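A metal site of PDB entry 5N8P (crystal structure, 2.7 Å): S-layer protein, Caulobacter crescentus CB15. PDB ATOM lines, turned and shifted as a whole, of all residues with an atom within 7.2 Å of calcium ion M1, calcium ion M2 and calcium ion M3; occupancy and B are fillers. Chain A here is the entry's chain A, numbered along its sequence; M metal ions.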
ATOM      1  N   VAL A 613     -12.808  -8.795  -9.605  1.00  0.00           N
ATOM      2  CA  VAL A 613     -12.857  -9.685 -10.754  1.00  0.00           C
ATOM      3  C   VAL A 613     -12.433  -8.981 -12.026  1.00  0.00           C
ATOM      4  O   VAL A 613     -12.861  -7.899 -12.358  1.00  0.00           O
ATOM      5  CB  VAL A 613     -14.235 -10.307 -10.948  1.00  0.00           C
ATOM      6  CG1 VAL A 613     -14.120 -11.485 -11.884  1.00  0.00           C
ATOM      7  CG2 VAL A 613     -14.772 -10.738  -9.599  1.00  0.00           C
ATOM      8  N   ASN A 615     -11.725 -11.367 -14.569  1.00  0.00           N
ATOM      9  CA  ASN A 615     -11.919 -12.564 -15.380  1.00  0.00           C
ATOM     10  C   ASN A 615     -12.953 -12.406 -16.495  1.00  0.00           C
ATOM     11  O   ASN A 615     -14.014 -11.893 -16.258  1.00  0.00           O
ATOM     12  CB  ASN A 615     -12.318 -13.715 -14.441  1.00  0.00           C
ATOM     13  CG  ASN A 615     -12.441 -15.053 -15.165  1.00  0.00           C
ATOM     14  OD1 ASN A 615     -13.281 -15.220 -16.041  1.00  0.00           O
ATOM     15  ND2 ASN A 615     -11.619 -16.016 -14.765  1.00  0.00           N
ATOM     16  N   VAL A 617     -14.831 -14.707 -18.355  1.00  0.00           N
ATOM     17  CA  VAL A 617     -16.086 -15.449 -18.259  1.00  0.00           C
ATOM     18  C   VAL A 617     -16.846 -14.943 -17.048  1.00  0.00           C
ATOM     19  O   VAL A 617     -18.052 -14.821 -17.078  1.00  0.00           O
ATOM     20  CB  VAL A 617     -15.839 -16.974 -18.281  1.00  0.00           C
ATOM     21  CG1 VAL A 617     -17.086 -17.786 -17.905  1.00  0.00           C
ATOM     22  CG2 VAL A 617     -15.318 -17.378 -19.655  1.00  0.00           C
ATOM     23  N   GLY A 618     -16.107 -14.622 -15.996  1.00  0.00           N
ATOM     24  CA  GLY A 618     -16.704 -14.108 -14.773  1.00  0.00           C
ATOM     25  C   GLY A 618     -16.377 -14.919 -13.555  1.00  0.00           C
ATOM     26  O   GLY A 618     -15.661 -15.917 -13.626  1.00  0.00           O
ATOM     27  N   PHE A 631     -16.857  -4.606  -3.888  1.00  0.00           N
ATOM     28  CA  PHE A 631     -16.725  -5.581  -4.947  1.00  0.00           C
ATOM     29  C   PHE A 631     -16.680  -4.890  -6.292  1.00  0.00           C
ATOM     30  O   PHE A 631     -17.459  -4.031  -6.547  1.00  0.00           O
ATOM     31  CB  PHE A 631     -17.901  -6.577  -4.913  1.00  0.00           C
ATOM     32  CG  PHE A 631     -17.884  -7.574  -6.054  1.00  0.00           C
ATOM     33  CD1 PHE A 631     -17.331  -8.834  -5.882  1.00  0.00           C
ATOM     34  CD2 PHE A 631     -18.393  -7.237  -7.315  1.00  0.00           C
ATOM     35  CE1 PHE A 631     -17.278  -9.743  -6.916  1.00  0.00           C
ATOM     36  CE2 PHE A 631     -18.352  -8.141  -8.367  1.00  0.00           C
ATOM     37  CZ  PHE A 631     -17.799  -9.392  -8.162  1.00  0.00           C
ATOM     38  N   THR A 632     -15.795  -5.323  -7.160  1.00  0.00           N
ATOM     39  CA  THR A 632     -15.729  -4.766  -8.518  1.00  0.00           C
ATOM     40  C   THR A 632     -15.709  -5.894  -9.561  1.00  0.00           C
ATOM     41  O   THR A 632     -14.815  -6.705  -9.552  1.00  0.00           O
ATOM     42  CB  THR A 632     -14.501  -3.836  -8.626  1.00  0.00           C
ATOM     43  OG1 THR A 632     -14.424  -3.041  -7.447  1.00  0.00           O
ATOM     44  CG2 THR A 632     -14.566  -2.962  -9.866  1.00  0.00           C
ATOM     45  N   GLY A 633     -16.722  -5.962 -10.416  1.00  0.00           N
ATOM     46  CA  GLY A 633     -16.743  -6.924 -11.535  1.00  0.00           C
ATOM     47  C   GLY A 633     -15.915  -6.441 -12.724  1.00  0.00           C
ATOM     48  O   GLY A 633     -15.395  -5.306 -12.714  1.00  0.00           O
ATOM     49  N   GLY A 634     -15.785  -7.288 -13.745  1.00  0.00           N
ATOM     50  CA  GLY A 634     -15.124  -6.938 -15.028  1.00  0.00           C
ATOM     51  C   GLY A 634     -16.086  -7.258 -16.129  1.00  0.00           C
ATOM     52  O   GLY A 634     -17.302  -7.260 -15.871  1.00  0.00           O
ATOM     53  N   ALA A 635     -15.617  -7.526 -17.358  1.00  0.00           N
ATOM     54  CA  ALA A 635     -16.474  -8.120 -18.405  1.00  0.00           C
ATOM     55  C   ALA A 635     -16.978  -9.472 -17.889  1.00  0.00           C
ATOM     56  O   ALA A 635     -16.516  -9.946 -16.873  1.00  0.00           O
ATOM     57  CB  ALA A 635     -15.732  -8.253 -19.739  1.00  0.00           C
ATOM     58  N   GLY A 636     -17.960 -10.062 -18.553  1.00  0.00           N
ATOM     59  CA  GLY A 636     -18.405 -11.403 -18.154  1.00  0.00           C
ATOM     60  C   GLY A 636     -19.226 -11.547 -16.885  1.00  0.00           C
ATOM     61  O   GLY A 636     -19.112 -10.759 -15.932  1.00  0.00           O
ATOM     62  N   ALA A 637     -20.042 -12.597 -16.874  1.00  0.00           N
ATOM     63  CA  ALA A 637     -21.129 -12.786 -15.922  1.00  0.00           C
ATOM     64  C   ALA A 637     -20.598 -12.943 -14.517  1.00  0.00           C
ATOM     65  O   ALA A 637     -20.331 -14.053 -14.097  1.00  0.00           O
ATOM     66  CB  ALA A 637     -22.024 -13.979 -16.320  1.00  0.00           C
ATOM     67  N   ASP A 638     -20.394 -11.847 -13.805  1.00  0.00           N
ATOM     68  CA  ASP A 638     -20.002 -11.972 -12.411  1.00  0.00           C
ATOM     69  C   ASP A 638     -21.278 -12.146 -11.571  1.00  0.00           C
ATOM     70  O   ASP A 638     -22.360 -11.798 -12.047  1.00  0.00           O
ATOM     71  CB  ASP A 638     -19.104 -10.798 -11.966  1.00  0.00           C
ATOM     72  CG  ASP A 638     -18.013 -10.424 -13.007  1.00  0.00           C
ATOM     73  OD1 ASP A 638     -17.095 -11.214 -13.273  1.00  0.00           O
ATOM     74  OD2 ASP A 638     -18.085  -9.317 -13.579  1.00  0.00           O
ATOM     75  N   SER A 639     -21.190 -12.719 -10.360  1.00  0.00           N
ATOM     76  CA  SER A 639     -22.411 -13.054  -9.582  1.00  0.00           C
ATOM     77  C   SER A 639     -22.265 -13.233  -8.067  1.00  0.00           C
ATOM     78  O   SER A 639     -21.647 -14.192  -7.604  1.00  0.00           O
ATOM     79  CB  SER A 639     -23.131 -14.249 -10.174  1.00  0.00           C
ATOM     80  OG  SER A 639     -23.983 -14.823  -9.212  1.00  0.00           O
ATOM     81  N   VAL A 650     -19.791  -2.173  -7.954  1.00  0.00           N
ATOM     82  CA  VAL A 650     -19.859  -2.052  -9.407  1.00  0.00           C
ATOM     83  C   VAL A 650     -19.744  -3.432 -10.000  1.00  0.00           C
ATOM     84  O   VAL A 650     -19.063  -4.262  -9.452  1.00  0.00           O
ATOM     85  CB  VAL A 650     -18.785  -1.116 -10.038  1.00  0.00           C
ATOM     86  CG1 VAL A 650     -19.145  -0.803 -11.510  1.00  0.00           C
ATOM     87  CG2 VAL A 650     -18.671   0.184  -9.233  1.00  0.00           C
ATOM     88  N   MET A 651     -20.415  -3.668 -11.130  1.00  0.00           N
ATOM     89  CA  MET A 651     -20.538  -4.976 -11.682  1.00  0.00           C
ATOM     90  C   MET A 651     -19.868  -5.117 -13.019  1.00  0.00           C
ATOM     91  O   MET A 651     -19.711  -6.252 -13.496  1.00  0.00           O
ATOM     92  CB  MET A 651     -21.989  -5.335 -11.805  1.00  0.00           C
ATOM     93  CG  MET A 651     -22.356  -6.621 -11.136  1.00  0.00           C
ATOM     94  SD  MET A 651     -21.922  -6.607  -9.403  1.00  0.00           S
ATOM     95  CE  MET A 651     -22.088  -8.373  -9.057  1.00  0.00           C
ATOM     96  N   GLY A 652     -19.470  -3.992 -13.629  1.00  0.00           N
ATOM     97  CA  GLY A 652     -18.760  -4.000 -14.935  1.00  0.00           C
ATOM     98  C   GLY A 652     -19.640  -4.427 -16.101  1.00  0.00           C
ATOM     99  O   GLY A 652     -20.864  -4.467 -15.970  1.00  0.00           O
ATOM    100  N   ALA A 653     -19.020  -4.759 -17.234  1.00  0.00           N
ATOM    101  CA  ALA A 653     -19.743  -5.240 -18.431  1.00  0.00           C
ATOM    102  C   ALA A 653     -20.263  -6.681 -18.274  1.00  0.00           C
ATOM    103  O   ALA A 653     -20.115  -7.275 -17.214  1.00  0.00           O
ATOM    104  CB  ALA A 653     -18.884  -5.096 -19.701  1.00  0.00           C
ATOM    105  N   GLY A 654     -20.908  -7.213 -19.322  1.00  0.00           N
ATOM    106  CA  GLY A 654     -21.426  -8.581 -19.339  1.00  0.00           C
ATOM    107  C   GLY A 654     -22.632  -8.863 -18.461  1.00  0.00           C
ATOM    108  O   GLY A 654     -23.020  -8.045 -17.630  1.00  0.00           O
ATOM    109  N   ASP A 655     -23.222 -10.032 -18.598  1.00  0.00           N
ATOM    110  CA  ASP A 655     -24.500 -10.293 -17.980  1.00  0.00           C
ATOM    111  C   ASP A 655     -24.443 -10.758 -16.517  1.00  0.00           C
ATOM    112  O   ASP A 655     -24.435 -11.956 -16.200  1.00  0.00           O
ATOM    113  CB  ASP A 655     -25.309 -11.193 -18.908  1.00  0.00           C
ATOM    114  CG  ASP A 655     -25.580 -10.523 -20.258  1.00  0.00           C
ATOM    115  OD1 ASP A 655     -26.364 -11.134 -21.028  1.00  0.00           O
ATOM    116  OD2 ASP A 655     -25.042  -9.406 -20.566  1.00  0.00           O
ATOM    117  N   ASP A 656     -24.427  -9.766 -15.631  1.00  0.00           N
ATOM    118  CA  ASP A 656     -24.130  -9.976 -14.207  1.00  0.00           C
ATOM    119  C   ASP A 656     -25.361 -10.311 -13.381  1.00  0.00           C
ATOM    120  O   ASP A 656     -26.470 -10.179 -13.874  1.00  0.00           O
ATOM    121  CB  ASP A 656     -23.468  -8.718 -13.671  1.00  0.00           C
ATOM    122  CG  ASP A 656     -22.109  -8.453 -14.298  1.00  0.00           C
ATOM    123  OD1 ASP A 656     -21.161  -9.235 -14.053  1.00  0.00           O
ATOM    124  OD2 ASP A 656     -21.949  -7.438 -15.024  1.00  0.00           O
ATOM    125  N   THR A 657     -25.178 -10.729 -12.129  1.00  0.00           N
ATOM    126  CA  THR A 657     -26.320 -11.136 -11.256  1.00  0.00           C
ATOM    127  C   THR A 657     -26.080 -10.819  -9.763  1.00  0.00           C
ATOM    128  O   THR A 657     -25.319 -11.539  -9.101  1.00  0.00           O
ATOM    129  CB  THR A 657     -26.602 -12.655 -11.364  1.00  0.00           C
ATOM    130  OG1 THR A 657     -26.663 -13.019 -12.730  1.00  0.00           O
ATOM    131  CG2 THR A 657     -27.982 -12.992 -10.743  1.00  0.00           C
ATOM    132  N   ASN A 672     -24.373  -0.795  -8.917  1.00  0.00           N
ATOM    133  CA  ASN A 672     -24.626  -0.550 -10.314  1.00  0.00           C
ATOM    134  C   ASN A 672     -24.303  -1.802 -11.147  1.00  0.00           C
ATOM    135  O   ASN A 672     -23.183  -2.277 -11.139  1.00  0.00           O
ATOM    136  CB  ASN A 672     -23.876   0.725 -10.798  1.00  0.00           C
ATOM    137  CG  ASN A 672     -23.867   0.882 -12.339  1.00  0.00           C
ATOM    138  OD1 ASN A 672     -24.871   0.708 -13.019  1.00  0.00           O
ATOM    139  ND2 ASN A 672     -22.716   1.254 -12.881  1.00  0.00           N
ATOM    140  N   GLY A 673     -25.304  -2.342 -11.834  1.00  0.00           N
ATOM    141  CA  GLY A 673     -25.141  -3.422 -12.785  1.00  0.00           C
ATOM    142  C   GLY A 673     -24.208  -3.203 -13.968  1.00  0.00           C
ATOM    143  O   GLY A 673     -23.851  -4.184 -14.620  1.00  0.00           O
ATOM    144  N   GLY A 674     -23.790  -1.948 -14.261  1.00  0.00           N
ATOM    145  CA  GLY A 674     -22.930  -1.622 -15.428  1.00  0.00           C
ATOM    146  C   GLY A 674     -23.557  -1.994 -16.792  1.00  0.00           C
ATOM    147  O   GLY A 674     -24.752  -2.219 -16.894  1.00  0.00           O
ATOM    148  N   ASP A 675     -22.750  -2.049 -17.838  1.00  0.00           N
ATOM    149  CA  ASP A 675     -23.225  -2.444 -19.175  1.00  0.00           C
ATOM    150  C   ASP A 675     -23.739  -3.891 -19.267  1.00  0.00           C
ATOM    151  O   ASP A 675     -23.365  -4.747 -18.444  1.00  0.00           O
ATOM    152  CB  ASP A 675     -22.127  -2.276 -20.230  1.00  0.00           C
ATOM    153  CG  ASP A 675     -21.661  -0.857 -20.399  1.00  0.00           C
ATOM    154  OD1 ASP A 675     -22.073   0.010 -19.568  1.00  0.00           O
ATOM    155  OD2 ASP A 675     -20.876  -0.641 -21.358  1.00  0.00           O
ATOM    156  N   GLY A 676     -24.579  -4.146 -20.281  1.00  0.00           N
ATOM    157  CA  GLY A 676     -25.123  -5.493 -20.553  1.00  0.00           C
ATOM    158  C   GLY A 676     -26.426  -5.782 -19.832  1.00  0.00           C
ATOM    159  O   GLY A 676     -26.925  -4.945 -19.069  1.00  0.00           O
ATOM    160  N   THR A 677     -26.986  -6.959 -20.063  1.00  0.00           N
ATOM    161  CA  THR A 677     -28.273  -7.291 -19.469  1.00  0.00           C
ATOM    162  C   THR A 677     -28.013  -7.933 -18.137  1.00  0.00           C
ATOM    163  O   THR A 677     -27.529  -9.066 -18.073  1.00  0.00           O
ATOM    164  CB  THR A 677     -29.076  -8.227 -20.387  1.00  0.00           C
ATOM    165  OG1 THR A 677     -29.021  -7.696 -21.715  1.00  0.00           O
ATOM    166  CG2 THR A 677     -30.527  -8.301 -19.956  1.00  0.00           C
ATOM    167  N   ASP A 678     -28.346  -7.226 -17.058  1.00  0.00           N
ATOM    168  CA  ASP A 678     -27.995  -7.690 -15.714  1.00  0.00           C
ATOM    169  C   ASP A 678     -29.221  -8.002 -14.912  1.00  0.00           C
ATOM    170  O   ASP A 678     -30.175  -7.244 -14.941  1.00  0.00           O
ATOM    171  CB  ASP A 678     -27.163  -6.631 -14.988  1.00  0.00           C
ATOM    172  CG  ASP A 678     -26.036  -6.081 -15.837  1.00  0.00           C
ATOM    173  OD1 ASP A 678     -25.000  -6.778 -15.974  1.00  0.00           O
ATOM    174  OD2 ASP A 678     -26.176  -4.930 -16.348  1.00  0.00           O
ATOM    175  N   GLY A 696     -28.917   0.825 -10.031  1.00  0.00           N
ATOM    176  CA  GLY A 696     -28.954   1.321 -11.420  1.00  0.00           C
ATOM    177  C   GLY A 696     -28.328   0.312 -12.380  1.00  0.00           C
ATOM    178  O   GLY A 696     -27.566  -0.567 -11.928  1.00  0.00           O
ATOM    179  N   GLY A 697     -28.625   0.404 -13.684  1.00  0.00           N
ATOM    180  CA  GLY A 697     -27.986  -0.497 -14.678  1.00  0.00           C
ATOM    181  C   GLY A 697     -28.498  -1.927 -14.756  1.00  0.00           C
ATOM    182  O   GLY A 697     -27.925  -2.782 -15.451  1.00  0.00           O
ATOM    183  N   PHE A 698     -29.598  -2.198 -14.045  1.00  0.00           N
ATOM    184  CA  PHE A 698     -30.295  -3.489 -14.101  1.00  0.00           C
ATOM    185  C   PHE A 698     -31.416  -3.519 -15.148  1.00  0.00           C
ATOM    186  O   PHE A 698     -32.001  -2.495 -15.449  1.00  0.00           O
ATOM    187  CB  PHE A 698     -30.807  -3.867 -12.701  1.00  0.00           C
ATOM    188  CG  PHE A 698     -29.705  -4.242 -11.770  1.00  0.00           C
ATOM    189  CD1 PHE A 698     -29.175  -5.540 -11.791  1.00  0.00           C
ATOM    190  CD2 PHE A 698     -29.138  -3.296 -10.933  1.00  0.00           C
ATOM    191  CE1 PHE A 698     -28.110  -5.882 -10.964  1.00  0.00           C
ATOM    192  CE2 PHE A 698     -28.090  -3.634 -10.100  1.00  0.00           C
ATOM    193  CZ  PHE A 698     -27.568  -4.931 -10.127  1.00  0.00           C
ATOM    194  N   GLU A 699     -31.672  -4.697 -15.701  1.00  0.00           N
ATOM    195  CA  GLU A 699     -32.607  -4.835 -16.820  1.00  0.00           C
ATOM    196  C   GLU A 699     -33.661  -5.870 -16.528  1.00  0.00           C
ATOM    197  O   GLU A 699     -34.726  -5.808 -17.117  1.00  0.00           O
ATOM    198  CB  GLU A 699     -31.862  -5.205 -18.094  1.00  0.00           C
ATOM    199  CG  GLU A 699     -31.107  -4.062 -18.740  1.00  0.00           C
ATOM    200  CD  GLU A 699     -29.774  -3.732 -18.072  1.00  0.00           C
ATOM    201  OE1 GLU A 699     -29.200  -4.521 -17.270  1.00  0.00           O
ATOM    202  OE2 GLU A 699     -29.255  -2.624 -18.370  1.00  0.00           O
HETATM  203 CA    CA M   1     -19.198  -8.148 -15.069  1.00  0.00          CA
HETATM  204 CA    CA M   2     -22.974  -5.816 -16.303  1.00  0.00          CA
HETATM  205 CA    CA M   3     -27.060  -2.899 -17.697  1.00  0.00          CA
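Along chain A the residues within 4 Å of calcium ion M3 span positions 674 to 699.
The nearest printed residue that does not touch calcium ion M3 is Phe 698 (4.5 Å).
Calcium ion M1 is bound by OD2 of Asp 638 (2.2 Å), O of Gly 634 (2.2 Å), OD1 of Asp 656 (2.5 Å), O of Ala 653 (2.5 Å), O of Met 651 (2.5 Å), O of Gly 636 (2.8 Å) and OD2 of Asp 656 (2.8 Å).
Calcium ion M1 has seven donor atoms within binding distance.
Within 4 Å of calcium ion M2: Gly 652, Ala 653, Gly 654, Asp 656, Gly 673, Gly 674, Asp 675 and Asp 678.
The nearest printed residue that does not touch calcium ion M2 is Met 651 (4.3 Å).
Residues that only touch calcium ion M1: Ala 635 (3.7 Å).
OE2 of Glu 699 is bound to calcium ion M3, at 2.3 Å.
Calcium ion M3 is bound by the backbone carbonyl oxygen (O) of Gly 697 (2.4 Å).
The backbone carbonyl oxygen (O) of Gly 676 binds calcium ion M3 (2.5 Å).
Calcium ion M3 is bound by O of Gly 674 (2.5 Å).
The side-chain carboxylate (OD2) of Asp 678 is bound to calcium ion M3 (2.6 Å).
Calcium ion M3 is bound by OE1 of Glu 699 (2.7 Å).
The backbone carbonyl oxygen (O) of Asp 638 sits at hydrogen-bond distance from the backbone NH (N) of Thr 657.
The backbone carbonyl oxygen (O) of Val 613 lies within hydrogen-bond range of the backbone NH (N) of Gly 634 (3.3 Å).
N of Gly 673 lies within hydrogen-bond range of O of Gly 696, at 2.9 Å.
O of Asn 672 is in hydrogen-bond range of N of Met 651 (3.1 Å).
The side-chain amide oxygen of Asn 672 sits at hydrogen-bond distance from the backbone NH of Gly 674, at 3.1 Å.
Calcium ion M2 is bound by the side-chain carboxylate of Asp 678 (2.3 Å), the side-chain carboxylate of Asp 656 (2.3 Å), the backbone carbonyl oxygen of Asp 675 (2.4 Å), the backbone carbonyl oxygen of Gly 673 (2.5 Å), the backbone carbonyl oxygen of Gly 652 (2.5 Å) and the backbone carbonyl oxygen of Gly 654 (2.6 Å).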
